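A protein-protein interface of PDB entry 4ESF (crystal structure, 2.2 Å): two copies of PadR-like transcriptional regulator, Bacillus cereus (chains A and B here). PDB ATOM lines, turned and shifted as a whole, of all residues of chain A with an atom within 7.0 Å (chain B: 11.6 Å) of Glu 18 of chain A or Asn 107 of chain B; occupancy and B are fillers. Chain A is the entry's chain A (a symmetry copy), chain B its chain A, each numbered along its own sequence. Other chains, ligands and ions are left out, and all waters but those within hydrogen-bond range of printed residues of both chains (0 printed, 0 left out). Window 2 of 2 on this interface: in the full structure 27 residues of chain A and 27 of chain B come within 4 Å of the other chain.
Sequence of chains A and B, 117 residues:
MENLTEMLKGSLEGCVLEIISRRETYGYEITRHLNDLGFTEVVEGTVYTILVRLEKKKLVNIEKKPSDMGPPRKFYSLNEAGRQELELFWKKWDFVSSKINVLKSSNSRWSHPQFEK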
ATOM      1  N   LEU A  12      11.333  14.519 -30.916  1.00  0.00           N
ATOM      2  CA  LEU A  12      10.037  14.389 -30.321  1.00  0.00           C
ATOM      3  C   LEU A  12      10.057  14.634 -28.806  1.00  0.00           C
ATOM      4  O   LEU A  12       9.133  15.239 -28.240  1.00  0.00           O
ATOM      5  CB  LEU A  12       9.496  13.010 -30.642  1.00  0.00           C
ATOM      6  CG  LEU A  12       8.005  12.885 -30.360  1.00  0.00           C
ATOM      7  CD1 LEU A  12       7.245  13.941 -31.136  1.00  0.00           C
ATOM      8  CD2 LEU A  12       7.537  11.474 -30.716  1.00  0.00           C
ATOM      9  N   GLU A  13      11.109  14.176 -28.141  1.00  0.00           N
ATOM     10  CA  GLU A  13      11.235  14.423 -26.708  1.00  0.00           C
ATOM     11  C   GLU A  13      11.224  15.924 -26.408  1.00  0.00           C
ATOM     12  O   GLU A  13      10.550  16.365 -25.467  1.00  0.00           O
ATOM     13  CB  GLU A  13      12.503  13.765 -26.149  1.00  0.00           C
ATOM     14  CG  GLU A  13      12.766  14.120 -24.710  1.00  0.00           C
ATOM     15  CD  GLU A  13      13.965  13.398 -24.148  1.00  0.00           C
ATOM     16  OE1 GLU A  13      14.049  12.170 -24.360  1.00  0.00           O
ATOM     17  OE2 GLU A  13      14.832  14.067 -23.534  1.00  0.00           O
ATOM     18  N   GLY A  14      11.939  16.699 -27.226  1.00  0.00           N
ATOM     19  CA  GLY A  14      11.955  18.150 -27.093  1.00  0.00           C
ATOM     20  C   GLY A  14      10.598  18.823 -27.325  1.00  0.00           C
ATOM     21  O   GLY A  14      10.211  19.762 -26.612  1.00  0.00           O
ATOM     22  N   CYS A  15       9.875  18.370 -28.338  1.00  0.00           N
ATOM     23  CA  CYS A  15       8.536  18.899 -28.600  1.00  0.00           C
ATOM     24  C   CYS A  15       7.648  18.658 -27.372  1.00  0.00           C
ATOM     25  O   CYS A  15       6.915  19.534 -26.949  1.00  0.00           O
ATOM     26  CB  CYS A  15       7.955  18.248 -29.859  1.00  0.00           C
ATOM     27  SG  CYS A  15       8.844  18.711 -31.357  1.00  0.00           S
ATOM     28  N   VAL A  16       7.765  17.484 -26.770  1.00  0.00           N
ATOM     29  CA  VAL A  16       7.009  17.183 -25.558  1.00  0.00           C
ATOM     30  C   VAL A  16       7.371  18.109 -24.394  1.00  0.00           C
ATOM     31  O   VAL A  16       6.479  18.699 -23.756  1.00  0.00           O
ATOM     32  CB  VAL A  16       7.184  15.709 -25.144  1.00  0.00           C
ATOM     33  CG1 VAL A  16       6.576  15.472 -23.779  1.00  0.00           C
ATOM     34  CG2 VAL A  16       6.560  14.781 -26.207  1.00  0.00           C
ATOM     35  N   LEU A  17       8.673  18.252 -24.135  1.00  0.00           N
ATOM     36  CA  LEU A  17       9.150  19.198 -23.126  1.00  0.00           C
ATOM     37  C   LEU A  17       8.579  20.581 -23.389  1.00  0.00           C
ATOM     38  O   LEU A  17       8.119  21.264 -22.477  1.00  0.00           O
ATOM     39  CB  LEU A  17      10.677  19.275 -23.130  1.00  0.00           C
ATOM     40  CG  LEU A  17      11.417  18.190 -22.390  1.00  0.00           C
ATOM     41  CD1 LEU A  17      12.934  18.172 -22.783  1.00  0.00           C
ATOM     42  CD2 LEU A  17      11.233  18.423 -20.905  1.00  0.00           C
ATOM     43  N   GLU A  18       8.606  21.001 -24.646  1.00  0.00           N
ATOM     44  CA  GLU A  18       8.065  22.298 -24.981  1.00  0.00           C
ATOM     45  C   GLU A  18       6.568  22.375 -24.618  1.00  0.00           C
ATOM     46  O   GLU A  18       6.124  23.374 -24.061  1.00  0.00           O
ATOM     47  CB  GLU A  18       8.276  22.624 -26.464  1.00  0.00           C
ATOM     48  CG  GLU A  18       7.480  23.869 -26.934  1.00  0.00           C
ATOM     49  CD  GLU A  18       7.950  25.114 -26.234  1.00  0.00           C
ATOM     50  OE1 GLU A  18       9.176  25.184 -25.951  1.00  0.00           O
ATOM     51  OE2 GLU A  18       7.120  26.010 -25.950  1.00  0.00           O
ATOM     52  N   ILE A  19       5.804  21.320 -24.923  1.00  0.00           N
ATOM     53  CA  ILE A  19       4.365  21.310 -24.630  1.00  0.00           C
ATOM     54  C   ILE A  19       4.130  21.355 -23.113  1.00  0.00           C
ATOM     55  O   ILE A  19       3.340  22.161 -22.632  1.00  0.00           O
ATOM     56  CB  ILE A  19       3.636  20.067 -25.256  1.00  0.00           C
ATOM     57  CG1 ILE A  19       3.566  20.185 -26.784  1.00  0.00           C
ATOM     58  CG2 ILE A  19       2.205  19.959 -24.721  1.00  0.00           C
ATOM     59  CD1 ILE A  19       3.274  18.877 -27.519  1.00  0.00           C
ATOM     60  N   ILE A  20       4.845  20.513 -22.361  1.00  0.00           N
ATOM     61  CA  ILE A  20       4.675  20.486 -20.911  1.00  0.00           C
ATOM     62  C   ILE A  20       5.040  21.824 -20.253  1.00  0.00           C
ATOM     63  O   ILE A  20       4.507  22.169 -19.193  1.00  0.00           O
ATOM     64  CB  ILE A  20       5.536  19.392 -20.277  1.00  0.00           C
ATOM     65  CG1 ILE A  20       5.083  18.027 -20.776  1.00  0.00           C
ATOM     66  CG2 ILE A  20       5.457  19.479 -18.756  1.00  0.00           C
ATOM     67  CD1 ILE A  20       6.085  16.898 -20.542  1.00  0.00           C
ATOM     68  N   SER A  21       5.945  22.568 -20.887  1.00  0.00           N
ATOM     69  CA  SER A  21       6.421  23.830 -20.341  1.00  0.00           C
ATOM     70  C   SER A  21       5.323  24.866 -20.246  1.00  0.00           C
ATOM     71  O   SER A  21       5.352  25.726 -19.358  1.00  0.00           O
ATOM     72  CB  SER A  21       7.572  24.391 -21.194  1.00  0.00           C
ATOM     73  OG  SER A  21       7.105  25.141 -22.314  1.00  0.00           O
ATOM     74  N   ARG A  22       4.358  24.804 -21.166  1.00  0.00           N
ATOM     75  CA  ARG A  22       3.339  25.849 -21.276  1.00  0.00           C
ATOM     76  C   ARG A  22       2.335  25.794 -20.126  1.00  0.00           C
ATOM     77  O   ARG A  22       1.740  26.820 -19.761  1.00  0.00           O
ATOM     78  CB  ARG A  22       2.602  25.727 -22.616  1.00  0.00           C
ATOM     79  CG  ARG A  22       3.568  25.487 -23.757  1.00  0.00           C
ATOM     80  CD  ARG A  22       3.078  25.995 -25.074  1.00  0.00           C
ATOM     81  NE  ARG A  22       4.205  26.178 -25.981  1.00  0.00           N
ATOM     82  CZ  ARG A  22       4.088  26.504 -27.265  1.00  0.00           C
ATOM     83  NH1 ARG A  22       2.883  26.689 -27.820  1.00  0.00           N
ATOM     84  NH2 ARG A  22       5.188  26.647 -27.996  1.00  0.00           N
ATOM     85  N   ARG A  23       2.152  24.593 -19.574  1.00  0.00           N
ATOM     86  CA  ARG A  23       1.318  24.388 -18.390  1.00  0.00           C
ATOM     87  C   ARG A  23       1.184  22.908 -18.031  1.00  0.00           C
ATOM     88  O   ARG A  23       1.421  22.023 -18.856  1.00  0.00           O
ATOM     89  CB  ARG A  23      -0.067  25.017 -18.571  1.00  0.00           C
ATOM     90  CG  ARG A  23      -0.861  24.501 -19.744  1.00  0.00           C
ATOM     91  CD  ARG A  23      -2.294  25.026 -19.654  1.00  0.00           C
ATOM     92  NE  ARG A  23      -3.148  24.494 -20.713  1.00  0.00           N
ATOM     93  CZ  ARG A  23      -3.664  23.269 -20.718  1.00  0.00           C
ATOM     94  NH1 ARG A  23      -3.418  22.425 -19.719  1.00  0.00           N
ATOM     95  NH2 ARG A  23      -4.424  22.882 -21.735  1.00  0.00           N
ATOM     96  N   LEU A  78       7.245  21.081 -15.823  1.00  0.00           N
ATOM     97  CA  LEU A  78       8.710  21.126 -15.870  1.00  0.00           C
ATOM     98  C   LEU A  78       9.296  21.544 -14.536  1.00  0.00           C
ATOM     99  O   LEU A  78       8.799  22.459 -13.905  1.00  0.00           O
ATOM    100  CB  LEU A  78       9.195  22.106 -16.948  1.00  0.00           C
ATOM    101  CG  LEU A  78       8.958  21.691 -18.401  1.00  0.00           C
ATOM    102  CD1 LEU A  78       9.724  22.610 -19.308  1.00  0.00           C
ATOM    103  CD2 LEU A  78       9.321  20.233 -18.657  1.00  0.00           C
ATOM    104  N   LEU A  86      15.160  21.903 -22.049  1.00  0.00           N
ATOM    105  CA  LEU A  86      14.348  22.443 -23.160  1.00  0.00           C
ATOM    106  C   LEU A  86      15.125  23.549 -23.878  1.00  0.00           C
ATOM    107  O   LEU A  86      15.106  23.642 -25.102  1.00  0.00           O
ATOM    108  CB  LEU A  86      13.015  23.019 -22.646  1.00  0.00           C
ATOM    109  CG  LEU A  86      12.109  23.701 -23.686  1.00  0.00           C
ATOM    110  CD1 LEU A  86      11.697  22.723 -24.773  1.00  0.00           C
ATOM    111  CD2 LEU A  86      10.834  24.327 -23.061  1.00  0.00           C
ATOM    112  N   GLU A  87      15.788  24.399 -23.112  1.00  0.00           N
ATOM    113  CA  GLU A  87      16.618  25.432 -23.724  1.00  0.00           C
ATOM    114  C   GLU A  87      17.697  24.794 -24.591  1.00  0.00           C
ATOM    115  O   GLU A  87      17.958  25.254 -25.682  1.00  0.00           O
ATOM    116  CB  GLU A  87      17.274  26.327 -22.674  1.00  0.00           C
ATOM    117  CG  GLU A  87      16.301  27.184 -21.866  1.00  0.00           C
ATOM    118  CD  GLU A  87      17.019  28.119 -20.887  1.00  0.00           C
ATOM    119  OE1 GLU A  87      16.621  28.186 -19.699  1.00  0.00           O
ATOM    120  OE2 GLU A  87      17.976  28.789 -21.316  1.00  0.00           O
ATOM    121  N   PHE A  89      17.661  21.909 -26.034  1.00  0.00           N
ATOM    122  CA  PHE A  89      17.034  21.261 -27.185  1.00  0.00           C
ATOM    123  C   PHE A  89      16.821  22.261 -28.313  1.00  0.00           C
ATOM    124  O   PHE A  89      17.120  21.972 -29.456  1.00  0.00           O
ATOM    125  CB  PHE A  89      15.678  20.658 -26.788  1.00  0.00           C
ATOM    126  CG  PHE A  89      14.789  20.372 -27.958  1.00  0.00           C
ATOM    127  CD1 PHE A  89      15.043  19.273 -28.796  1.00  0.00           C
ATOM    128  CD2 PHE A  89      13.696  21.178 -28.218  1.00  0.00           C
ATOM    129  CE1 PHE A  89      14.216  18.990 -29.887  1.00  0.00           C
ATOM    130  CE2 PHE A  89      12.847  20.908 -29.306  1.00  0.00           C
ATOM    131  CZ  PHE A  89      13.100  19.813 -30.141  1.00  0.00           C
ATOM    132  N   TRP A  90      16.279  23.430 -27.985  1.00  0.00           N
ATOM    133  CA  TRP A  90      15.995  24.437 -28.995  1.00  0.00           C
ATOM    134  C   TRP A  90      17.308  24.974 -29.596  1.00  0.00           C
ATOM    135  O   TRP A  90      17.359  25.265 -30.789  1.00  0.00           O
ATOM    136  CB  TRP A  90      15.134  25.584 -28.431  1.00  0.00           C
ATOM    137  CG  TRP A  90      13.644  25.230 -28.300  1.00  0.00           C
ATOM    138  CD1 TRP A  90      12.863  25.311 -27.166  1.00  0.00           C
ATOM    139  CD2 TRP A  90      12.789  24.730 -29.341  1.00  0.00           C
ATOM    140  NE1 TRP A  90      11.573  24.880 -27.451  1.00  0.00           N
ATOM    141  CE2 TRP A  90      11.507  24.521 -28.774  1.00  0.00           C
ATOM    142  CE3 TRP A  90      12.986  24.430 -30.694  1.00  0.00           C
ATOM    143  CZ2 TRP A  90      10.421  24.042 -29.529  1.00  0.00           C
ATOM    144  CZ3 TRP A  90      11.911  23.938 -31.440  1.00  0.00           C
ATOM    145  CH2 TRP A  90      10.645  23.750 -30.854  1.00  0.00           C
ATOM    146  N   MET B   7      19.567  13.767 -32.924  1.00  0.00           N
ATOM    147  CA  MET B   7      18.719  14.687 -33.676  1.00  0.00           C
ATOM    148  C   MET B   7      19.021  14.634 -35.167  1.00  0.00           C
ATOM    149  O   MET B   7      18.118  14.701 -36.004  1.00  0.00           O
ATOM    150  CB  MET B   7      18.911  16.114 -33.161  1.00  0.00           C
ATOM    151  CG  MET B   7      18.038  17.151 -33.854  1.00  0.00           C
ATOM    152  SD  MET B   7      18.194  18.778 -33.081  1.00  0.00           S
ATOM    153  CE  MET B   7      17.328  18.558 -31.514  1.00  0.00           C
ATOM    154  N   LYS B  99       6.657  22.448 -38.775  1.00  0.00           N
ATOM    155  CA  LYS B  99       5.728  22.222 -37.668  1.00  0.00           C
ATOM    156  C   LYS B  99       6.440  22.354 -36.342  1.00  0.00           C
ATOM    157  O   LYS B  99       5.883  22.845 -35.360  1.00  0.00           O
ATOM    158  CB  LYS B  99       5.029  20.859 -37.797  1.00  0.00           C
ATOM    159  CG  LYS B  99       4.138  20.725 -39.048  1.00  0.00           C
ATOM    160  CD  LYS B  99       3.485  22.061 -39.405  1.00  0.00           C
ATOM    161  CE  LYS B  99       2.786  22.021 -40.757  1.00  0.00           C
ATOM    162  NZ  LYS B  99       1.795  20.935 -40.789  1.00  0.00           N
ATOM    163  N   ILE B 100       7.685  21.908 -36.303  1.00  0.00           N
ATOM    164  CA  ILE B 100       8.504  22.142 -35.127  1.00  0.00           C
ATOM    165  C   ILE B 100       8.768  23.642 -34.907  1.00  0.00           C
ATOM    166  O   ILE B 100       8.688  24.122 -33.778  1.00  0.00           O
ATOM    167  CB  ILE B 100       9.794  21.361 -35.232  1.00  0.00           C
ATOM    168  CG1 ILE B 100       9.468  19.879 -35.021  1.00  0.00           C
ATOM    169  CG2 ILE B 100      10.834  21.906 -34.236  1.00  0.00           C
ATOM    170  CD1 ILE B 100      10.614  18.947 -35.299  1.00  0.00           C
ATOM    171  N   ASN B 101       9.056  24.384 -35.971  1.00  0.00           N
ATOM    172  CA  ASN B 101       9.167  25.830 -35.852  1.00  0.00           C
ATOM    173  C   ASN B 101       7.865  26.551 -35.463  1.00  0.00           C
ATOM    174  O   ASN B 101       7.915  27.612 -34.824  1.00  0.00           O
ATOM    175  CB  ASN B 101       9.731  26.436 -37.132  1.00  0.00           C
ATOM    176  CG  ASN B 101      11.205  26.118 -37.316  1.00  0.00           C
ATOM    177  OD1 ASN B 101      11.923  25.868 -36.344  1.00  0.00           O
ATOM    178  ND2 ASN B 101      11.659  26.118 -38.563  1.00  0.00           N
ATOM    179  N   VAL B 102       6.713  26.006 -35.859  1.00  0.00           N
ATOM    180  CA  VAL B 102       5.420  26.586 -35.460  1.00  0.00           C
ATOM    181  C   VAL B 102       5.306  26.458 -33.948  1.00  0.00           C
ATOM    182  O   VAL B 102       4.792  27.334 -33.259  1.00  0.00           O
ATOM    183  CB  VAL B 102       4.238  25.885 -36.166  1.00  0.00           C
ATOM    184  CG1 VAL B 102       2.920  26.128 -35.411  1.00  0.00           C
ATOM    185  CG2 VAL B 102       4.136  26.354 -37.619  1.00  0.00           C
ATOM    186  N   LEU B 103       5.839  25.363 -33.438  1.00  0.00           N
ATOM    187  CA  LEU B 103       5.814  25.084 -32.015  1.00  0.00           C
ATOM    188  C   LEU B 103       6.796  25.974 -31.249  1.00  0.00           C
ATOM    189  O   LEU B 103       6.476  26.516 -30.195  1.00  0.00           O
ATOM    190  CB  LEU B 103       6.154  23.622 -31.805  1.00  0.00           C
ATOM    191  CG  LEU B 103       5.950  23.097 -30.396  1.00  0.00           C
ATOM    192  CD1 LEU B 103       4.470  23.104 -29.996  1.00  0.00           C
ATOM    193  CD2 LEU B 103       6.520  21.719 -30.321  1.00  0.00           C
ATOM    194  N   LYS B 104       8.001  26.104 -31.785  1.00  0.00           N
ATOM    195  CA  LYS B 104       9.009  26.973 -31.212  1.00  0.00           C
ATOM    196  C   LYS B 104       8.485  28.401 -31.163  1.00  0.00           C
ATOM    197  O   LYS B 104       8.742  29.130 -30.207  1.00  0.00           O
ATOM    198  CB  LYS B 104      10.280  26.937 -32.069  1.00  0.00           C
ATOM    199  CG  LYS B 104      11.443  27.754 -31.524  1.00  0.00           C
ATOM    200  CD  LYS B 104      12.626  27.709 -32.475  1.00  0.00           C
ATOM    201  CE  LYS B 104      12.483  28.725 -33.595  1.00  0.00           C
ATOM    202  NZ  LYS B 104      13.380  28.439 -34.761  1.00  0.00           N
ATOM    203  N   SER B 105       7.743  28.793 -32.197  1.00  0.00           N
ATOM    204  CA  SER B 105       7.301  30.181 -32.340  1.00  0.00           C
ATOM    205  C   SER B 105       6.526  30.705 -31.130  1.00  0.00           C
ATOM    206  O   SER B 105       6.295  31.906 -31.022  1.00  0.00           O
ATOM    207  CB  SER B 105       6.468  30.360 -33.607  1.00  0.00           C
ATOM    208  OG  SER B 105       7.263  30.138 -34.752  1.00  0.00           O
ATOM    209  N   SER B 106       6.136  29.826 -30.218  1.00  0.00           N
ATOM    210  CA  SER B 106       5.415  30.265 -29.027  1.00  0.00           C
ATOM    211  C   SER B 106       6.256  30.124 -27.744  1.00  0.00           C
ATOM    212  O   SER B 106       5.728  30.195 -26.634  1.00  0.00           O
ATOM    213  CB  SER B 106       4.070  29.544 -28.923  1.00  0.00           C
ATOM    214  OG  SER B 106       3.313  29.733 -30.113  1.00  0.00           O
ATOM    215  N   ASN B 107       7.561  29.911 -27.920  1.00  0.00           N
ATOM    216  CA  ASN B 107       8.581  30.343 -26.948  1.00  0.00           C
ATOM    217  C   ASN B 107       9.999  30.216 -27.510  1.00  0.00           C
ATOM    218  O   ASN B 107      10.554  31.176 -28.055  1.00  0.00           O
ATOM    219  CB  ASN B 107       8.491  29.608 -25.615  1.00  0.00           C
ATOM    220  CG  ASN B 107       9.484  30.160 -24.586  1.00  0.00           C
ATOM    221  OD1 ASN B 107      10.698  29.950 -24.695  1.00  0.00           O
ATOM    222  ND2 ASN B 107       8.968  30.880 -23.591  1.00  0.00           N
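The backbone carbonyl oxygen (O) of Leu 103 of chain B is in hydrogen-bond range of the guanidinium group (NH2) of Arg 22 of chain A, 2.6 Å away.
NZ of Lys 104 of chain B sits at hydrogen-bond distance from OD1 of Asn 101 of chain B, at 3.4 Å.
O of Glu 18 of chain A is in hydrogen-bond range of OG of Ser 21 of chain A, 2.7 Å away.
NH2 of Arg 22 of chain A is in salt-bridge range of OE2 of Glu 18 of chain A (2.9 Å).
The side-chain carboxylate (OE1) of Glu 18 of chain A is in hydrogen-bond range of the indole nitrogen (NE1) of Trp 90 of chain A.
Among the printed residues, merely in contact across the chains: Arg 22 of chain A with Ser 106 of chain B, Trp 90 of chain A with Lys 104 of chain B, Trp 90 of chain A with Ile 100 of chain B, Phe 89 of chain A with Met 7 of chain B, Cys 15 of chain A with Leu 103 of chain B, Glu 18 of chain A with Leu 103 of chain B, Glu 18 of chain A with Asn 107 of chain B and Cys 15 of chain A with Ile 100 of chain B.
No residue of chain B comes within 4 Å of Val 16 of chain A.
Leu 17 of chain A touches none of the printed residues of chain B.
Of chain B, only Leu 103 (3.9 Å) and Asn 107 (3.9 Å) come within 4 Å of Glu 18 of chain A.
Ile 20 of chain A touches none of the printed residues of chain B.
No residue of chain B comes within 4 Å of Ser 21 of chain A.
No residue of chain B comes within 4 Å of Leu 86 of chain A.
Of the printed residues of chain B, Phe 89 of chain A touches Met 7 (3.5 Å).
Lys 99 of chain B touches none of the printed residues of chain A.
Asn 101 of chain B touches none of the printed residues of chain A.
Of the printed residues of chain A, Leu 103 of chain B touches Cys 15 (3.8 Å), Glu 18 (3.9 Å) and Arg 22 (2.6 Å).
Of the printed residues of chain A, Ser 106 of chain B touches Arg 22 (3.2 Å).
Of chain A, only Glu 18 (3.9 Å) comes within 4 Å of Asn 107 of chain B.
Of the 10 printed residues of chain B, 6 touch a printed residue of chain A.
Of the 17 printed residues of chain A, 5 touch a printed residue of chain B.
Among the printed residues, 9 pairs touch across the chains.
No position is printed for both chains.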
